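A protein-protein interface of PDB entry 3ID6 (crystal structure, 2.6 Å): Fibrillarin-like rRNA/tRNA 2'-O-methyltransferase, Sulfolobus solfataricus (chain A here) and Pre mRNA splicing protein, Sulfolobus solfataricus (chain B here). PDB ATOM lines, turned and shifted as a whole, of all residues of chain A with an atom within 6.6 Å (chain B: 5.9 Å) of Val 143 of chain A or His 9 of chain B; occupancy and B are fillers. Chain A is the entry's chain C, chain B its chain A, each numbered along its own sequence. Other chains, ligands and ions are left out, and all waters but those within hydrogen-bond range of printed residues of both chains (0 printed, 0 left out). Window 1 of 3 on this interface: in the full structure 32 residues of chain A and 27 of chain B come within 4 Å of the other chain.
ND2 of Asn 28 of chain B lies within hydrogen-bond range of O of Val 10 of chain B (2.9 Å). The side-chain hydroxyl (OH) of Tyr 105 of chain A lies within hydrogen-bond range of the side-chain carboxylate (OE2) of Glu 145 of chain A. NE2 of His 9 of chain B is in hydrogen-bond range of OH of Tyr 113 of chain B, at 3.5 Å. N of Phe 48 of chain B lies within hydrogen-bond range of OE2 of Glu 8 of chain B (3.1 Å). N of Glu 8 of chain B is in hydrogen-bond range of OE1 of Glu 66 of chain B (3.3 Å). The backbone carbonyl oxygen (O) of Leu 117 of chain B is in hydrogen-bond range of the side-chain hydroxyl (OG) of Ser 121 of chain B.
A ring nitrogen (ND1) of His 9 of chain B sits at hydrogen-bond distance from the backbone carbonyl oxygen of Ser 142 of chain A (3.2 Å). OH of Tyr 124 of chain B is in hydrogen-bond range of O of Ser 139 of chain A, at 3.3 Å. The side-chain carboxylate (OE2) of Glu 66 of chain B is in salt-bridge range of the side-chain amino group (NZ) of Lys 141 of chain A, at 2.8 Å. The backbone NH (N) of Val 10 of chain B lies within hydrogen-bond range of the backbone carbonyl oxygen (O) of Ser 142 of chain A, 2.8 Å away. The guanidinium group (NH2) of Arg 94 of chain B lies close to the side-chain amino group (NZ) of Lys 141 of chain A, 2.7 Å away. The side-chain hydroxyl (OG) of Ser 142 of chain A is in hydrogen-bond range of the backbone carbonyl oxygen (O) of Glu 8 of chain B (2.9 Å).
Among the printed residues, merely in contact across the chains: Tyr 105 of chain A with Leu 117 of chain B, Phe 128 of chain A with Leu 117 of chain B, Phe 128 of chain A with Ser 121 of chain B, Leu 130 of chain A with Tyr 124 of chain B, Lys 141 of chain A with His 9 of chain B, Ser 142 of chain A with Leu 39 of chain B, Val 143 of chain A with His 9 of chain B, Val 143 of chain A with Val 10 of chain B, Val 143 of chain A with Leu 39 of chain B, Val 144 of chain A with His 9 of chain B, Val 144 of chain A with Leu 97 of chain B, Glu 145 of chain A with Arg 94 of chain B and Glu 145 of chain A with Leu 97 of chain B.
Of chain B, only His 9 (3.6 Å), Val 10 (3.95 Å) and Leu 39 (3.97 Å) come within 4 Å of Val 143 of chain A. His 9 of chain B touches just these residues of chain A: Lys 141, Ser 142, Val 143 and Val 144. Printed residues of chain A within 4 Å of Val 10 of chain B: Ser 142 and Val 143. Of the printed residues of chain B, Val 144 of chain A touches His 9 (3.1 Å) and Leu 97 (3.2 Å). Of the printed residues of chain A, Arg 94 of chain B touches Lys 141 and Glu 145. Asn 28 of chain B touches none of the printed residues of chain A. Tyr 113 of chain B touches none of the printed residues of chain A. The nearest residue of chain B that does not touch Val 143 of chain A is Leu 117 of chain B (4.03 Å). The nearest residue of chain A that does not touch His 9 of chain B is Glu 145 of chain A (5.3 Å).
Hydrophobic or aromatic side chains of chain B within 4 Å of the printed part of chain A: His 9, Val 10, Leu 39, Leu 97, Leu 117 and Tyr 124. Printed residues of chain A that touch a printed residue of chain B: Tyr 105, Phe 128, Leu 130, Ser 139, Lys 141, Ser 142, Val 143, Val 144 and Glu 145. Hydrophobic or aromatic side chains of chain A within 4 Å of the printed part of chain B: Tyr 105, Phe 128, Leu 130 and Val 143. Along chain A the printed residues that touch a printed residue of chain B span positions 105 to 145. Among the printed residues, 19 pairs touch across the chains.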
ATOM      1  N   TYR A 105     -16.694  28.203   5.202  1.00  0.00           N
ATOM      2  CA  TYR A 105     -16.334  28.051   6.614  1.00  0.00           C
ATOM      3  C   TYR A 105     -16.369  29.426   7.281  1.00  0.00           C
ATOM      4  O   TYR A 105     -15.595  30.315   6.907  1.00  0.00           O
ATOM      5  CB  TYR A 105     -14.954  27.376   6.758  1.00  0.00           C
ATOM      6  CG  TYR A 105     -14.884  26.008   6.094  1.00  0.00           C
ATOM      7  CD1 TYR A 105     -14.477  25.870   4.773  1.00  0.00           C
ATOM      8  CD2 TYR A 105     -15.266  24.864   6.782  1.00  0.00           C
ATOM      9  CE1 TYR A 105     -14.433  24.610   4.149  1.00  0.00           C
ATOM     10  CE2 TYR A 105     -15.229  23.608   6.181  1.00  0.00           C
ATOM     11  CZ  TYR A 105     -14.811  23.484   4.865  1.00  0.00           C
ATOM     12  OH  TYR A 105     -14.779  22.226   4.279  1.00  0.00           O
ATOM     13  N   PHE A 128     -20.541  26.301   7.383  1.00  0.00           N
ATOM     14  CA  PHE A 128     -19.936  25.618   8.526  1.00  0.00           C
ATOM     15  C   PHE A 128     -19.459  26.658   9.549  1.00  0.00           C
ATOM     16  O   PHE A 128     -18.368  27.213   9.394  1.00  0.00           O
ATOM     17  CB  PHE A 128     -18.760  24.741   8.052  1.00  0.00           C
ATOM     18  CG  PHE A 128     -19.156  23.678   7.055  1.00  0.00           C
ATOM     19  CD1 PHE A 128     -19.199  23.955   5.690  1.00  0.00           C
ATOM     20  CD2 PHE A 128     -19.483  22.399   7.476  1.00  0.00           C
ATOM     21  CE1 PHE A 128     -19.575  22.971   4.761  1.00  0.00           C
ATOM     22  CE2 PHE A 128     -19.865  21.407   6.539  1.00  0.00           C
ATOM     23  CZ  PHE A 128     -19.903  21.706   5.193  1.00  0.00           C
ATOM     24  N   LEU A 130     -18.114  28.462  13.052  1.00  0.00           N
ATOM     25  CA  LEU A 130     -17.154  28.173  14.113  1.00  0.00           C
ATOM     26  C   LEU A 130     -16.959  29.337  15.070  1.00  0.00           C
ATOM     27  O   LEU A 130     -16.571  30.433  14.658  1.00  0.00           O
ATOM     28  CB  LEU A 130     -15.812  27.758  13.518  1.00  0.00           C
ATOM     29  CG  LEU A 130     -15.802  26.539  12.587  1.00  0.00           C
ATOM     30  CD1 LEU A 130     -14.650  26.626  11.603  1.00  0.00           C
ATOM     31  CD2 LEU A 130     -15.767  25.240  13.389  1.00  0.00           C
ATOM     32  N   SER A 139      -6.789  26.541  16.069  1.00  0.00           N
ATOM     33  CA  SER A 139      -7.975  26.137  16.831  1.00  0.00           C
ATOM     34  C   SER A 139      -9.192  25.785  15.957  1.00  0.00           C
ATOM     35  O   SER A 139     -10.267  25.468  16.492  1.00  0.00           O
ATOM     36  CB  SER A 139      -8.356  27.219  17.850  1.00  0.00           C
ATOM     37  OG  SER A 139      -8.844  28.390  17.200  1.00  0.00           O
ATOM     38  N   TYR A 140      -9.046  25.858  14.631  1.00  0.00           N
ATOM     39  CA  TYR A 140     -10.079  25.316  13.727  1.00  0.00           C
ATOM     40  C   TYR A 140      -9.484  24.528  12.543  1.00  0.00           C
ATOM     41  O   TYR A 140     -10.200  24.012  11.696  1.00  0.00           O
ATOM     42  CB  TYR A 140     -11.078  26.391  13.272  1.00  0.00           C
ATOM     43  CG  TYR A 140     -10.467  27.700  12.836  1.00  0.00           C
ATOM     44  CD1 TYR A 140     -10.132  27.926  11.507  1.00  0.00           C
ATOM     45  CD2 TYR A 140     -10.228  28.711  13.758  1.00  0.00           C
ATOM     46  CE1 TYR A 140      -9.572  29.122  11.110  1.00  0.00           C
ATOM     47  CE2 TYR A 140      -9.672  29.915  13.375  1.00  0.00           C
ATOM     48  CZ  TYR A 140      -9.344  30.122  12.052  1.00  0.00           C
ATOM     49  OH  TYR A 140      -8.784  31.333  11.681  1.00  0.00           O
ATOM     50  N   LYS A 141      -8.161  24.443  12.536  1.00  0.00           N
ATOM     51  CA  LYS A 141      -7.362  23.633  11.625  1.00  0.00           C
ATOM     52  C   LYS A 141      -7.813  22.168  11.552  1.00  0.00           C
ATOM     53  O   LYS A 141      -7.676  21.509  10.522  1.00  0.00           O
ATOM     54  CB  LYS A 141      -5.920  23.693  12.123  1.00  0.00           C
ATOM     55  CG  LYS A 141      -4.879  23.146  11.187  1.00  0.00           C
ATOM     56  CD  LYS A 141      -3.580  22.840  11.957  1.00  0.00           C
ATOM     57  CE  LYS A 141      -2.335  22.950  11.062  1.00  0.00           C
ATOM     58  NZ  LYS A 141      -2.222  21.823  10.111  1.00  0.00           N
ATOM     59  N   SER A 142      -8.337  21.658  12.660  1.00  0.00           N
ATOM     60  CA  SER A 142      -8.794  20.279  12.719  1.00  0.00           C
ATOM     61  C   SER A 142     -10.175  20.066  12.080  1.00  0.00           C
ATOM     62  O   SER A 142     -10.688  18.941  12.074  1.00  0.00           O
ATOM     63  CB  SER A 142      -8.799  19.793  14.169  1.00  0.00           C
ATOM     64  OG  SER A 142      -7.482  19.683  14.680  1.00  0.00           O
ATOM     65  N   VAL A 143     -10.764  21.138  11.546  1.00  0.00           N
ATOM     66  CA  VAL A 143     -12.135  21.100  11.010  1.00  0.00           C
ATOM     67  C   VAL A 143     -12.228  21.578   9.565  1.00  0.00           C
ATOM     68  O   VAL A 143     -12.882  20.938   8.742  1.00  0.00           O
ATOM     69  CB  VAL A 143     -13.132  21.922  11.871  1.00  0.00           C
ATOM     70  CG1 VAL A 143     -14.471  22.061  11.149  1.00  0.00           C
ATOM     71  CG2 VAL A 143     -13.334  21.273  13.232  1.00  0.00           C
ATOM     72  N   VAL A 144     -11.586  22.701   9.262  1.00  0.00           N
ATOM     73  CA  VAL A 144     -11.631  23.263   7.916  1.00  0.00           C
ATOM     74  C   VAL A 144     -10.832  22.434   6.901  1.00  0.00           C
ATOM     75  O   VAL A 144     -10.602  21.245   7.091  1.00  0.00           O
ATOM     76  CB  VAL A 144     -11.172  24.749   7.877  1.00  0.00           C
ATOM     77  CG1 VAL A 144     -12.114  25.619   8.689  1.00  0.00           C
ATOM     78  CG2 VAL A 144      -9.772  24.863   8.392  1.00  0.00           C
ATOM     79  N   GLU A 145     -10.386  23.098   5.843  1.00  0.00           N
ATOM     80  CA  GLU A 145      -9.941  22.461   4.625  1.00  0.00           C
ATOM     81  C   GLU A 145      -9.272  23.615   3.911  1.00  0.00           C
ATOM     82  O   GLU A 145      -9.497  24.766   4.288  1.00  0.00           O
ATOM     83  CB  GLU A 145     -11.187  22.036   3.851  1.00  0.00           C
ATOM     84  CG  GLU A 145     -10.988  21.081   2.701  1.00  0.00           C
ATOM     85  CD  GLU A 145     -12.212  21.012   1.780  1.00  0.00           C
ATOM     86  OE1 GLU A 145     -12.121  20.327   0.737  1.00  0.00           O
ATOM     87  OE2 GLU A 145     -13.257  21.635   2.091  1.00  0.00           O
ATOM     88  N   ILE B   7      -0.870  14.679  11.604  1.00  0.00           N
ATOM     89  CA  ILE B   7      -2.092  15.388  11.227  1.00  0.00           C
ATOM     90  C   ILE B   7      -3.242  14.866  12.093  1.00  0.00           C
ATOM     91  O   ILE B   7      -3.433  13.653  12.226  1.00  0.00           O
ATOM     92  CB  ILE B   7      -2.380  15.273   9.699  1.00  0.00           C
ATOM     93  CG1 ILE B   7      -1.755  16.450   8.938  1.00  0.00           C
ATOM     94  CG2 ILE B   7      -3.866  15.265   9.418  1.00  0.00           C
ATOM     95  CD1 ILE B   7      -0.227  16.356   8.713  1.00  0.00           C
ATOM     96  N   GLU B   8      -3.961  15.789  12.720  1.00  0.00           N
ATOM     97  CA  GLU B   8      -5.079  15.461  13.598  1.00  0.00           C
ATOM     98  C   GLU B   8      -6.277  16.251  13.126  1.00  0.00           C
ATOM     99  O   GLU B   8      -6.315  17.481  13.235  1.00  0.00           O
ATOM    100  CB  GLU B   8      -4.764  15.823  15.050  1.00  0.00           C
ATOM    101  CG  GLU B   8      -4.032  14.742  15.839  1.00  0.00           C
ATOM    102  CD  GLU B   8      -3.523  15.236  17.194  1.00  0.00           C
ATOM    103  OE1 GLU B   8      -2.930  16.338  17.236  1.00  0.00           O
ATOM    104  OE2 GLU B   8      -3.698  14.524  18.217  1.00  0.00           O
ATOM    105  N   HIS B   9      -7.247  15.542  12.577  1.00  0.00           N
ATOM    106  CA  HIS B   9      -8.390  16.178  11.977  1.00  0.00           C
ATOM    107  C   HIS B   9      -9.625  15.516  12.561  1.00  0.00           C
ATOM    108  O   HIS B   9      -9.527  14.499  13.255  1.00  0.00           O
ATOM    109  CB  HIS B   9      -8.322  15.980  10.454  1.00  0.00           C
ATOM    110  CG  HIS B   9      -9.273  16.836   9.673  1.00  0.00           C
ATOM    111  ND1 HIS B   9      -9.031  18.165   9.409  1.00  0.00           N
ATOM    112  CD2 HIS B   9     -10.458  16.544   9.083  1.00  0.00           C
ATOM    113  CE1 HIS B   9     -10.034  18.664   8.706  1.00  0.00           C
ATOM    114  NE2 HIS B   9     -10.914  17.702   8.498  1.00  0.00           N
ATOM    115  N   VAL B  10     -10.779  16.123  12.305  1.00  0.00           N
ATOM    116  CA  VAL B  10     -12.061  15.458  12.439  1.00  0.00           C
ATOM    117  C   VAL B  10     -12.018  13.992  11.974  1.00  0.00           C
ATOM    118  O   VAL B  10     -12.577  13.131  12.641  1.00  0.00           O
ATOM    119  CB  VAL B  10     -13.156  16.244  11.658  1.00  0.00           C
ATOM    120  CG1 VAL B  10     -14.291  15.338  11.189  1.00  0.00           C
ATOM    121  CG2 VAL B  10     -13.685  17.401  12.513  1.00  0.00           C
ATOM    122  N   ILE B  11     -11.352  13.709  10.851  1.00  0.00           N
ATOM    123  CA  ILE B  11     -11.379  12.351  10.277  1.00  0.00           C
ATOM    124  C   ILE B  11     -10.607  11.309  11.102  1.00  0.00           C
ATOM    125  O   ILE B  11     -10.867  10.117  10.992  1.00  0.00           O
ATOM    126  CB  ILE B  11     -10.953  12.293   8.767  1.00  0.00           C
ATOM    127  CG1 ILE B  11      -9.481  12.689   8.574  1.00  0.00           C
ATOM    128  CG2 ILE B  11     -11.890  13.124   7.916  1.00  0.00           C
ATOM    129  CD1 ILE B  11      -8.930  12.424   7.165  1.00  0.00           C
ATOM    130  N   GLY B  12      -9.674  11.771  11.931  1.00  0.00           N
ATOM    131  CA  GLY B  12      -8.851  10.881  12.735  1.00  0.00           C
ATOM    132  C   GLY B  12      -7.404  11.322  12.823  1.00  0.00           C
ATOM    133  O   GLY B  12      -7.081  12.500  12.605  1.00  0.00           O
ATOM    134  N   ALA B  13      -6.535  10.368  13.157  1.00  0.00           N
ATOM    135  CA  ALA B  13      -5.103  10.626  13.286  1.00  0.00           C
ATOM    136  C   ALA B  13      -4.354  10.032  12.104  1.00  0.00           C
ATOM    137  O   ALA B  13      -4.372   8.812  11.908  1.00  0.00           O
ATOM    138  CB  ALA B  13      -4.575  10.050  14.593  1.00  0.00           C
ATOM    139  N   ASN B  28     -11.099   8.201  13.325  1.00  0.00           N
ATOM    140  CA  ASN B  28     -12.064   8.497  14.376  1.00  0.00           C
ATOM    141  C   ASN B  28     -13.361   7.694  14.227  1.00  0.00           C
ATOM    142  O   ASN B  28     -13.741   7.335  13.105  1.00  0.00           O
ATOM    143  CB  ASN B  28     -12.397   9.992  14.379  1.00  0.00           C
ATOM    144  CG  ASN B  28     -11.515  10.786  15.314  1.00  0.00           C
ATOM    145  OD1 ASN B  28     -10.792  10.234  16.146  1.00  0.00           O
ATOM    146  ND2 ASN B  28     -11.578  12.092  15.190  1.00  0.00           N
ATOM    147  N   ILE B  35     -15.965  13.126  18.924  1.00  0.00           N
ATOM    148  CA  ILE B  35     -15.138  14.013  18.115  1.00  0.00           C
ATOM    149  C   ILE B  35     -15.164  15.440  18.671  1.00  0.00           C
ATOM    150  O   ILE B  35     -14.109  16.063  18.812  1.00  0.00           O
ATOM    151  CB  ILE B  35     -15.491  13.944  16.616  1.00  0.00           C
ATOM    152  CG1 ILE B  35     -15.437  12.490  16.138  1.00  0.00           C
ATOM    153  CG2 ILE B  35     -14.516  14.775  15.797  1.00  0.00           C
ATOM    154  CD1 ILE B  35     -15.835  12.302  14.683  1.00  0.00           C
ATOM    155  N   LEU B  39     -11.844  17.300  20.134  1.00  0.00           N
ATOM    156  CA  LEU B  39     -11.364  18.558  19.555  1.00  0.00           C
ATOM    157  C   LEU B  39     -11.169  19.650  20.603  1.00  0.00           C
ATOM    158  O   LEU B  39     -10.324  20.528  20.432  1.00  0.00           O
ATOM    159  CB  LEU B  39     -12.330  19.069  18.485  1.00  0.00           C
ATOM    160  CG  LEU B  39     -12.545  18.265  17.202  1.00  0.00           C
ATOM    161  CD1 LEU B  39     -13.664  18.887  16.382  1.00  0.00           C
ATOM    162  CD2 LEU B  39     -11.276  18.154  16.385  1.00  0.00           C
ATOM    163  N   PHE B  48      -5.356  13.320  20.520  1.00  0.00           N
ATOM    164  CA  PHE B  48      -6.478  12.416  20.286  1.00  0.00           C
ATOM    165  C   PHE B  48      -6.139  11.065  20.871  1.00  0.00           C
ATOM    166  O   PHE B  48      -4.971  10.662  20.854  1.00  0.00           O
ATOM    167  CB  PHE B  48      -6.720  12.214  18.789  1.00  0.00           C
ATOM    168  CG  PHE B  48      -7.412  13.360  18.107  1.00  0.00           C
ATOM    169  CD1 PHE B  48      -7.999  14.392  18.840  1.00  0.00           C
ATOM    170  CD2 PHE B  48      -7.508  13.383  16.721  1.00  0.00           C
ATOM    171  CE1 PHE B  48      -8.637  15.448  18.194  1.00  0.00           C
ATOM    172  CE2 PHE B  48      -8.150  14.428  16.071  1.00  0.00           C
ATOM    173  CZ  PHE B  48      -8.712  15.465  16.808  1.00  0.00           C
ATOM    174  N   GLU B  66       1.264  20.179  14.663  1.00  0.00           N
ATOM    175  CA  GLU B  66       0.616  21.408  14.201  1.00  0.00           C
ATOM    176  C   GLU B  66       0.350  22.426  15.336  1.00  0.00           C
ATOM    177  O   GLU B  66       0.258  23.630  15.080  1.00  0.00           O
ATOM    178  CB  GLU B  66      -0.701  21.048  13.502  1.00  0.00           C
ATOM    179  CG  GLU B  66      -0.587  19.920  12.464  1.00  0.00           C
ATOM    180  CD  GLU B  66      -1.927  19.238  12.124  1.00  0.00           C
ATOM    181  OE1 GLU B  66      -2.649  18.748  13.039  1.00  0.00           O
ATOM    182  OE2 GLU B  66      -2.244  19.172  10.918  1.00  0.00           O
ATOM    183  N   PHE B  93      -2.308  17.686   3.107  1.00  0.00           N
ATOM    184  CA  PHE B  93      -3.430  16.993   3.683  1.00  0.00           C
ATOM    185  C   PHE B  93      -4.759  17.718   3.412  1.00  0.00           C
ATOM    186  O   PHE B  93      -5.750  17.080   3.050  1.00  0.00           O
ATOM    187  CB  PHE B  93      -3.232  16.786   5.182  1.00  0.00           C
ATOM    188  CG  PHE B  93      -4.490  16.411   5.891  1.00  0.00           C
ATOM    189  CD1 PHE B  93      -5.046  15.147   5.719  1.00  0.00           C
ATOM    190  CD2 PHE B  93      -5.152  17.336   6.676  1.00  0.00           C
ATOM    191  CE1 PHE B  93      -6.231  14.795   6.355  1.00  0.00           C
ATOM    192  CE2 PHE B  93      -6.334  16.999   7.322  1.00  0.00           C
ATOM    193  CZ  PHE B  93      -6.876  15.725   7.161  1.00  0.00           C
ATOM    194  N   ARG B  94      -4.792  19.036   3.587  1.00  0.00           N
ATOM    195  CA  ARG B  94      -6.046  19.778   3.408  1.00  0.00           C
ATOM    196  C   ARG B  94      -6.479  19.925   1.940  1.00  0.00           C
ATOM    197  O   ARG B  94      -7.681  20.039   1.651  1.00  0.00           O
ATOM    198  CB  ARG B  94      -6.012  21.129   4.137  1.00  0.00           C
ATOM    199  CG  ARG B  94      -6.094  21.003   5.653  1.00  0.00           C
ATOM    200  CD  ARG B  94      -6.198  22.356   6.364  1.00  0.00           C
ATOM    201  NE  ARG B  94      -5.002  23.181   6.186  1.00  0.00           N
ATOM    202  CZ  ARG B  94      -3.925  23.131   6.965  1.00  0.00           C
ATOM    203  NH1 ARG B  94      -2.881  23.909   6.714  1.00  0.00           N
ATOM    204  NH2 ARG B  94      -3.883  22.295   7.988  1.00  0.00           N
ATOM    205  N   LEU B  97      -8.756  16.853   0.908  1.00  0.00           N
ATOM    206  CA  LEU B  97      -9.598  16.545   2.065  1.00  0.00           C
ATOM    207  C   LEU B  97     -11.030  16.052   1.851  1.00  0.00           C
ATOM    208  O   LEU B  97     -11.619  15.476   2.786  1.00  0.00           O
ATOM    209  CB  LEU B  97      -9.623  17.708   3.046  1.00  0.00           C
ATOM    210  CG  LEU B  97      -9.535  17.425   4.546  1.00  0.00           C
ATOM    211  CD1 LEU B  97     -10.130  18.614   5.265  1.00  0.00           C
ATOM    212  CD2 LEU B  97     -10.207  16.125   5.015  1.00  0.00           C
ATOM    213  N   TYR B 113     -19.585  12.742   4.013  1.00  0.00           N
ATOM    214  CA  TYR B 113     -18.512  13.446   4.708  1.00  0.00           C
ATOM    215  C   TYR B 113     -18.994  14.828   5.123  1.00  0.00           C
ATOM    216  O   TYR B 113     -18.930  15.181   6.309  1.00  0.00           O
ATOM    217  CB  TYR B 113     -17.232  13.556   3.867  1.00  0.00           C
ATOM    218  CG  TYR B 113     -16.209  14.498   4.481  1.00  0.00           C
ATOM    219  CD1 TYR B 113     -15.533  14.153   5.653  1.00  0.00           C
ATOM    220  CD2 TYR B 113     -15.942  15.744   3.905  1.00  0.00           C
ATOM    221  CE1 TYR B 113     -14.614  15.007   6.232  1.00  0.00           C
ATOM    222  CE2 TYR B 113     -15.015  16.620   4.473  1.00  0.00           C
ATOM    223  CZ  TYR B 113     -14.361  16.250   5.640  1.00  0.00           C
ATOM    224  OH  TYR B 113     -13.445  17.103   6.218  1.00  0.00           O
ATOM    225  N   LEU B 117     -19.731  16.590   8.516  1.00  0.00           N
ATOM    226  CA  LEU B 117     -18.964  17.785   8.849  1.00  0.00           C
ATOM    227  C   LEU B 117     -19.901  18.881   9.323  1.00  0.00           C
ATOM    228  O   LEU B 117     -19.619  19.563  10.302  1.00  0.00           O
ATOM    229  CB  LEU B 117     -18.196  18.284   7.629  1.00  0.00           C
ATOM    230  CG  LEU B 117     -16.720  18.678   7.718  1.00  0.00           C
ATOM    231  CD1 LEU B 117     -16.473  20.009   6.980  1.00  0.00           C
ATOM    232  CD2 LEU B 117     -16.222  18.732   9.171  1.00  0.00           C
ATOM    233  N   LEU B 120     -21.379  18.159  12.737  1.00  0.00           N
ATOM    234  CA  LEU B 120     -20.269  18.324  13.667  1.00  0.00           C
ATOM    235  C   LEU B 120     -20.039  19.775  14.096  1.00  0.00           C
ATOM    236  O   LEU B 120     -19.990  20.077  15.298  1.00  0.00           O
ATOM    237  CB  LEU B 120     -18.994  17.777  13.037  1.00  0.00           C
ATOM    238  CG  LEU B 120     -18.133  16.952  13.977  1.00  0.00           C
ATOM    239  CD1 LEU B 120     -17.101  16.228  13.151  1.00  0.00           C
ATOM    240  CD2 LEU B 120     -17.469  17.772  15.069  1.00  0.00           C
ATOM    241  N   SER B 121     -19.894  20.660  13.114  1.00  0.00           N
ATOM    242  CA  SER B 121     -19.670  22.075  13.363  1.00  0.00           C
ATOM    243  C   SER B 121     -20.814  22.717  14.151  1.00  0.00           C
ATOM    244  O   SER B 121     -20.580  23.607  14.962  1.00  0.00           O
ATOM    245  CB  SER B 121     -19.430  22.814  12.045  1.00  0.00           C
ATOM    246  OG  SER B 121     -20.576  22.766  11.214  1.00  0.00           O
ATOM    247  N   TYR B 124     -20.134  21.261  17.892  1.00  0.00           N
ATOM    248  CA  TYR B 124     -18.908  21.898  18.375  1.00  0.00           C
ATOM    249  C   TYR B 124     -19.089  23.365  18.783  1.00  0.00           C
ATOM    250  O   TYR B 124     -18.660  23.763  19.871  1.00  0.00           O
ATOM    251  CB  TYR B 124     -17.820  21.742  17.306  1.00  0.00           C
ATOM    252  CG  TYR B 124     -16.512  22.438  17.558  1.00  0.00           C
ATOM    253  CD1 TYR B 124     -15.623  21.981  18.524  1.00  0.00           C
ATOM    254  CD2 TYR B 124     -16.142  23.533  16.789  1.00  0.00           C
ATOM    255  CE1 TYR B 124     -14.394  22.615  18.733  1.00  0.00           C
ATOM    256  CE2 TYR B 124     -14.925  24.187  16.989  1.00  0.00           C
ATOM    257  CZ  TYR B 124     -14.053  23.721  17.959  1.00  0.00           C
ATOM    258  OH  TYR B 124     -12.854  24.379  18.152  1.00  0.00           O
